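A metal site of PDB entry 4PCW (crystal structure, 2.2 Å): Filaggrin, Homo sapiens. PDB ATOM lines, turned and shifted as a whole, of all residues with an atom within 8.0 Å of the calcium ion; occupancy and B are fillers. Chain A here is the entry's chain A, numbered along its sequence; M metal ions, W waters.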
ATOM      1  N   PHE A  17       7.045  -5.126 -21.104  1.00  0.00           N
ATOM      2  CA  PHE A  17       6.500  -4.171 -20.142  1.00  0.00           C
ATOM      3  C   PHE A  17       6.419  -4.784 -18.756  1.00  0.00           C
ATOM      4  O   PHE A  17       6.789  -4.158 -17.767  1.00  0.00           O
ATOM      5  CB  PHE A  17       5.128  -3.677 -20.595  1.00  0.00           C
ATOM      6  CG  PHE A  17       4.422  -2.802 -19.596  1.00  0.00           C
ATOM      7  CD1 PHE A  17       4.624  -1.441 -19.575  1.00  0.00           C
ATOM      8  CD2 PHE A  17       3.538  -3.358 -18.677  1.00  0.00           C
ATOM      9  CE1 PHE A  17       3.977  -0.631 -18.660  1.00  0.00           C
ATOM     10  CE2 PHE A  17       2.887  -2.560 -17.756  1.00  0.00           C
ATOM     11  CZ  PHE A  17       3.098  -1.195 -17.751  1.00  0.00           C
ATOM     12  N   LYS A  18       5.916  -6.012 -18.693  1.00  0.00           N
ATOM     13  CA  LYS A  18       5.708  -6.676 -17.417  1.00  0.00           C
ATOM     14  C   LYS A  18       7.030  -7.021 -16.733  1.00  0.00           C
ATOM     15  O   LYS A  18       7.081  -7.145 -15.504  1.00  0.00           O
ATOM     16  CB  LYS A  18       4.872  -7.941 -17.615  1.00  0.00           C
ATOM     17  CG  LYS A  18       3.472  -7.649 -18.133  1.00  0.00           C
ATOM     18  CD  LYS A  18       2.627  -8.896 -18.264  1.00  0.00           C
ATOM     19  CE  LYS A  18       2.063  -9.335 -16.915  1.00  0.00           C
ATOM     20  NZ  LYS A  18       0.697  -9.884 -17.060  1.00  0.00           N
ATOM     21  N   TYR A  20       9.507  -5.127 -16.367  1.00  0.00           N
ATOM     22  CA  TYR A  20       9.982  -3.979 -15.612  1.00  0.00           C
ATOM     23  C   TYR A  20       8.918  -3.457 -14.651  1.00  0.00           C
ATOM     24  O   TYR A  20       9.251  -2.870 -13.620  1.00  0.00           O
ATOM     25  CB  TYR A  20      10.437  -2.871 -16.571  1.00  0.00           C
ATOM     26  CG  TYR A  20      11.615  -3.259 -17.425  1.00  0.00           C
ATOM     27  CD1 TYR A  20      12.914  -3.181 -16.935  1.00  0.00           C
ATOM     28  CD2 TYR A  20      11.436  -3.724 -18.718  1.00  0.00           C
ATOM     29  CE1 TYR A  20      14.002  -3.542 -17.717  1.00  0.00           C
ATOM     30  CE2 TYR A  20      12.515  -4.095 -19.505  1.00  0.00           C
ATOM     31  CZ  TYR A  20      13.795  -4.000 -19.000  1.00  0.00           C
ATOM     32  OH  TYR A  20      14.861  -4.362 -19.781  1.00  0.00           O
ATOM     33  N   SER A  21       7.654  -3.664 -14.987  1.00  0.00           N
ATOM     34  CA  SER A  21       6.555  -3.159 -14.161  1.00  0.00           C
ATOM     35  C   SER A  21       6.349  -4.000 -12.918  1.00  0.00           C
ATOM     36  O   SER A  21       6.034  -3.481 -11.839  1.00  0.00           O
ATOM     37  CB  SER A  21       5.251  -3.116 -14.974  1.00  0.00           C
ATOM     38  OG  SER A  21       4.734  -4.415 -15.183  1.00  0.00           O
ATOM     39  N   LYS A  22       6.538  -5.315 -13.058  1.00  0.00           N
ATOM     40  CA  LYS A  22       6.299  -6.241 -11.963  1.00  0.00           C
ATOM     41  C   LYS A  22       7.504  -6.348 -11.031  1.00  0.00           C
ATOM     42  O   LYS A  22       7.609  -7.276 -10.237  1.00  0.00           O
ATOM     43  CB  LYS A  22       5.944  -7.626 -12.528  1.00  0.00           C
ATOM     44  CG  LYS A  22       4.727  -7.594 -13.446  1.00  0.00           C
ATOM     45  CD  LYS A  22       4.476  -8.937 -14.120  1.00  0.00           C
ATOM     46  CE  LYS A  22       4.097 -10.019 -13.128  1.00  0.00           C
ATOM     47  NZ  LYS A  22       3.207 -11.047 -13.733  1.00  0.00           N
ATOM     48  N   LYS A  23       8.409  -5.374 -11.127  1.00  0.00           N
ATOM     49  CA  LYS A  23       9.591  -5.323 -10.280  1.00  0.00           C
ATOM     50  C   LYS A  23       9.236  -4.919  -8.855  1.00  0.00           C
ATOM     51  O   LYS A  23      10.022  -5.150  -7.937  1.00  0.00           O
ATOM     52  CB  LYS A  23      10.613  -4.341 -10.851  1.00  0.00           C
ATOM     53  CG  LYS A  23      11.958  -4.953 -11.248  1.00  0.00           C
ATOM     54  CD  LYS A  23      12.301  -4.613 -12.686  1.00  0.00           C
ATOM     55  CE  LYS A  23      13.723  -5.041 -13.030  1.00  0.00           C
ATOM     56  NZ  LYS A  23      13.859  -6.528 -13.116  1.00  0.00           N
ATOM     57  N   ASP A  24       8.065  -4.326  -8.669  1.00  0.00           N
ATOM     58  CA  ASP A  24       7.666  -3.776  -7.376  1.00  0.00           C
ATOM     59  C   ASP A  24       6.265  -4.224  -6.970  1.00  0.00           C
ATOM     60  O   ASP A  24       5.722  -5.201  -7.498  1.00  0.00           O
ATOM     61  CB  ASP A  24       7.742  -2.244  -7.410  1.00  0.00           C
ATOM     62  CG  ASP A  24       6.611  -1.623  -8.205  1.00  0.00           C
ATOM     63  OD1 ASP A  24       6.084  -2.295  -9.113  1.00  0.00           O
ATOM     64  OD2 ASP A  24       6.256  -0.460  -7.917  1.00  0.00           O
ATOM     65  N   LYS A  25       5.686  -3.490  -6.023  1.00  0.00           N
ATOM     66  CA  LYS A  25       4.327  -3.735  -5.557  1.00  0.00           C
ATOM     67  C   LYS A  25       3.310  -3.394  -6.644  1.00  0.00           C
ATOM     68  O   LYS A  25       2.340  -4.127  -6.868  1.00  0.00           O
ATOM     69  CB  LYS A  25       4.051  -2.911  -4.308  1.00  0.00           C
ATOM     70  CG  LYS A  25       2.805  -3.312  -3.537  1.00  0.00           C
ATOM     71  CD  LYS A  25       3.132  -4.192  -2.331  1.00  0.00           C
ATOM     72  CE  LYS A  25       2.074  -4.068  -1.248  1.00  0.00           C
ATOM     73  NZ  LYS A  25       2.049  -2.705  -0.647  1.00  0.00           N
ATOM     74  N   ASN A  26       3.537  -2.278  -7.331  1.00  0.00           N
ATOM     75  CA  ASN A  26       2.666  -1.817  -8.398  1.00  0.00           C
ATOM     76  C   ASN A  26       2.977  -2.549  -9.703  1.00  0.00           C
ATOM     77  O   ASN A  26       3.758  -2.064 -10.518  1.00  0.00           O
ATOM     78  CB  ASN A  26       2.802  -0.308  -8.577  1.00  0.00           C
ATOM     79  CG  ASN A  26       2.620   0.457  -7.278  1.00  0.00           C
ATOM     80  OD1 ASN A  26       1.722   0.168  -6.487  1.00  0.00           O
ATOM     81  ND2 ASN A  26       3.493   1.441  -7.045  1.00  0.00           N
ATOM     82  N   THR A  27       2.360  -3.711  -9.893  1.00  0.00           N
ATOM     83  CA  THR A  27       2.755  -4.616 -10.969  1.00  0.00           C
ATOM     84  C   THR A  27       2.131  -4.303 -12.324  1.00  0.00           C
ATOM     85  O   THR A  27       2.628  -4.778 -13.356  1.00  0.00           O
ATOM     86  CB  THR A  27       2.401  -6.072 -10.596  1.00  0.00           C
ATOM     87  OG1 THR A  27       0.998  -6.163 -10.307  1.00  0.00           O
ATOM     88  CG2 THR A  27       3.198  -6.521  -9.382  1.00  0.00           C
ATOM     89  N   ASP A  28       1.059  -3.518 -12.347  1.00  0.00           N
ATOM     90  CA  ASP A  28       0.389  -3.162 -13.604  1.00  0.00           C
ATOM     91  C   ASP A  28       0.794  -1.776 -14.089  1.00  0.00           C
ATOM     92  O   ASP A  28       0.162  -1.221 -14.990  1.00  0.00           O
ATOM     93  CB  ASP A  28      -1.134  -3.233 -13.430  1.00  0.00           C
ATOM     94  CG  ASP A  28      -1.625  -4.648 -13.179  1.00  0.00           C
ATOM     95  OD1 ASP A  28      -0.874  -5.608 -13.438  1.00  0.00           O
ATOM     96  OD2 ASP A  28      -2.788  -4.805 -12.731  1.00  0.00           O
ATOM     97  N   THR A  29       1.845  -1.212 -13.499  1.00  0.00           N
ATOM     98  CA  THR A  29       2.357   0.098 -13.897  1.00  0.00           C
ATOM     99  C   THR A  29       3.866   0.174 -13.710  1.00  0.00           C
ATOM    100  O   THR A  29       4.439  -0.585 -12.924  1.00  0.00           O
ATOM    101  CB  THR A  29       1.718   1.241 -13.075  1.00  0.00           C
ATOM    102  OG1 THR A  29       2.022   1.080 -11.687  1.00  0.00           O
ATOM    103  CG2 THR A  29       0.213   1.290 -13.271  1.00  0.00           C
ATOM    104  N   LEU A  30       4.497   1.097 -14.428  1.00  0.00           N
ATOM    105  CA  LEU A  30       5.919   1.368 -14.261  1.00  0.00           C
ATOM    106  C   LEU A  30       6.124   2.563 -13.342  1.00  0.00           C
ATOM    107  O   LEU A  30       5.544   3.633 -13.556  1.00  0.00           O
ATOM    108  CB  LEU A  30       6.598   1.636 -15.617  1.00  0.00           C
ATOM    109  CG  LEU A  30       6.564   0.526 -16.659  1.00  0.00           C
ATOM    110  CD1 LEU A  30       6.770   1.101 -18.056  1.00  0.00           C
ATOM    111  CD2 LEU A  30       7.625  -0.515 -16.348  1.00  0.00           C
ATOM    112  N   SER A  31       6.952   2.395 -12.321  1.00  0.00           N
ATOM    113  CA  SER A  31       7.355   3.505 -11.475  1.00  0.00           C
ATOM    114  C   SER A  31       8.467   4.270 -12.189  1.00  0.00           C
ATOM    115  O   SER A  31       8.888   3.886 -13.278  1.00  0.00           O
ATOM    116  CB  SER A  31       7.837   3.015 -10.113  1.00  0.00           C
ATOM    117  OG  SER A  31       9.058   2.301 -10.239  1.00  0.00           O
ATOM    118  N   LYS A  32       8.926   5.351 -11.570  1.00  0.00           N
ATOM    119  CA  LYS A  32       9.965   6.177 -12.174  1.00  0.00           C
ATOM    120  C   LYS A  32      11.246   5.367 -12.389  1.00  0.00           C
ATOM    121  O   LYS A  32      11.850   5.419 -13.459  1.00  0.00           O
ATOM    122  CB  LYS A  32      10.250   7.392 -11.300  1.00  0.00           C
ATOM    123  CG  LYS A  32      11.104   8.445 -11.991  1.00  0.00           C
ATOM    124  CD  LYS A  32      11.474   9.564 -11.034  1.00  0.00           C
ATOM    125  CE  LYS A  32      11.812  10.835 -11.783  1.00  0.00           C
ATOM    126  NZ  LYS A  32      10.599  11.426 -12.420  1.00  0.00           N
ATOM    127  N   GLU A  34      11.573   2.096 -12.498  1.00  0.00           N
ATOM    128  CA  GLU A  34      11.337   0.980 -13.407  1.00  0.00           C
ATOM    129  C   GLU A  34      11.370   1.441 -14.859  1.00  0.00           C
ATOM    130  O   GLU A  34      11.903   0.744 -15.732  1.00  0.00           O
ATOM    131  CB  GLU A  34      10.006   0.315 -13.087  1.00  0.00           C
ATOM    132  CG  GLU A  34      10.002  -0.372 -11.731  1.00  0.00           C
ATOM    133  CD  GLU A  34       8.651  -0.896 -11.348  1.00  0.00           C
ATOM    134  OE1 GLU A  34       7.659  -0.496 -11.987  1.00  0.00           O
ATOM    135  OE2 GLU A  34       8.579  -1.731 -10.412  1.00  0.00           O
ATOM    136  N   LEU A  35      10.799   2.611 -15.118  1.00  0.00           N
ATOM    137  CA  LEU A  35      10.848   3.212 -16.444  1.00  0.00           C
ATOM    138  C   LEU A  35      12.299   3.492 -16.821  1.00  0.00           C
ATOM    139  O   LEU A  35      12.738   3.150 -17.915  1.00  0.00           O
ATOM    140  CB  LEU A  35      10.036   4.504 -16.497  1.00  0.00           C
ATOM    141  CG  LEU A  35      10.078   5.278 -17.827  1.00  0.00           C
ATOM    142  CD1 LEU A  35       9.610   4.420 -18.992  1.00  0.00           C
ATOM    143  CD2 LEU A  35       9.255   6.542 -17.731  1.00  0.00           C
ATOM    144  N   LYS A  70       2.697   7.101 -12.200  1.00  0.00           N
ATOM    145  CA  LYS A  70       2.886   5.734 -12.659  1.00  0.00           C
ATOM    146  C   LYS A  70       2.528   5.617 -14.140  1.00  0.00           C
ATOM    147  O   LYS A  70       1.664   6.347 -14.625  1.00  0.00           O
ATOM    148  CB  LYS A  70       2.043   4.760 -11.844  1.00  0.00           C
ATOM    149  CG  LYS A  70       2.650   4.395 -10.485  1.00  0.00           C
ATOM    150  CD  LYS A  70       1.775   4.853  -9.333  1.00  0.00           C
ATOM    151  CE  LYS A  70       0.458   4.104  -9.273  1.00  0.00           C
ATOM    152  NZ  LYS A  70      -0.658   4.952  -8.757  1.00  0.00           N
ATOM    153  N   ILE A  71       3.181   4.696 -14.844  1.00  0.00           N
ATOM    154  CA  ILE A  71       2.934   4.509 -16.268  1.00  0.00           C
ATOM    155  C   ILE A  71       2.266   3.174 -16.518  1.00  0.00           C
ATOM    156  O   ILE A  71       2.915   2.132 -16.503  1.00  0.00           O
ATOM    157  CB  ILE A  71       4.246   4.584 -17.089  1.00  0.00           C
ATOM    158  CG1 ILE A  71       5.030   5.852 -16.745  1.00  0.00           C
ATOM    159  CG2 ILE A  71       3.959   4.518 -18.569  1.00  0.00           C
ATOM    160  CD1 ILE A  71       4.279   7.148 -16.984  1.00  0.00           C
HETATM  161 CA    CA M   1       5.729  -0.884 -10.886  1.00  0.00          CA
HETATM  162  O   HOH W   1       4.600   1.398 -10.710  1.00  0.00           O
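Water W1 bridges OG1 of Thr 29 and N of Ser 31.
Residues that only touch the calcium ion: Ser 31 (3.8 Å).
Six residues have an atom within 4 Å of the calcium ion: Ser 21, Asp 24, Asn 26, Thr 29, Ser 31 and Glu 34.
The calcium ion is bound by OE1 of Glu 34, at 2.3 Å.
The calcium ion is bound by the side-chain carboxylate (OD1) of Asp 24 (2.3 Å).
The calcium ion is bound by O of Asn 26.
O of Thr 29 binds the calcium ion (2.4 Å).
The calcium ion is bound by water W1, 2.6 Å away.
The calcium ion is bound by O of Ser 21 (2.8 Å).
Slightly farther from the calcium ion lies OE2 of Glu 34 (3.0 Å).
Slightly farther from the calcium ion lies the side-chain carboxylate (OD2) of Asp 24 (3.0 Å).
The side-chain hydroxyl (OG) of Ser 21 is in hydrogen-bond range of the backbone carbonyl oxygen (O) of Phe 17 (3.3 Å).
OG of Ser 21 is in hydrogen-bond range of O of Thr 27 (2.8 Å).
The backbone NH (N) of Glu 34 sits close to the side-chain hydroxyl (OG) of Ser 31, 3.4 Å away.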
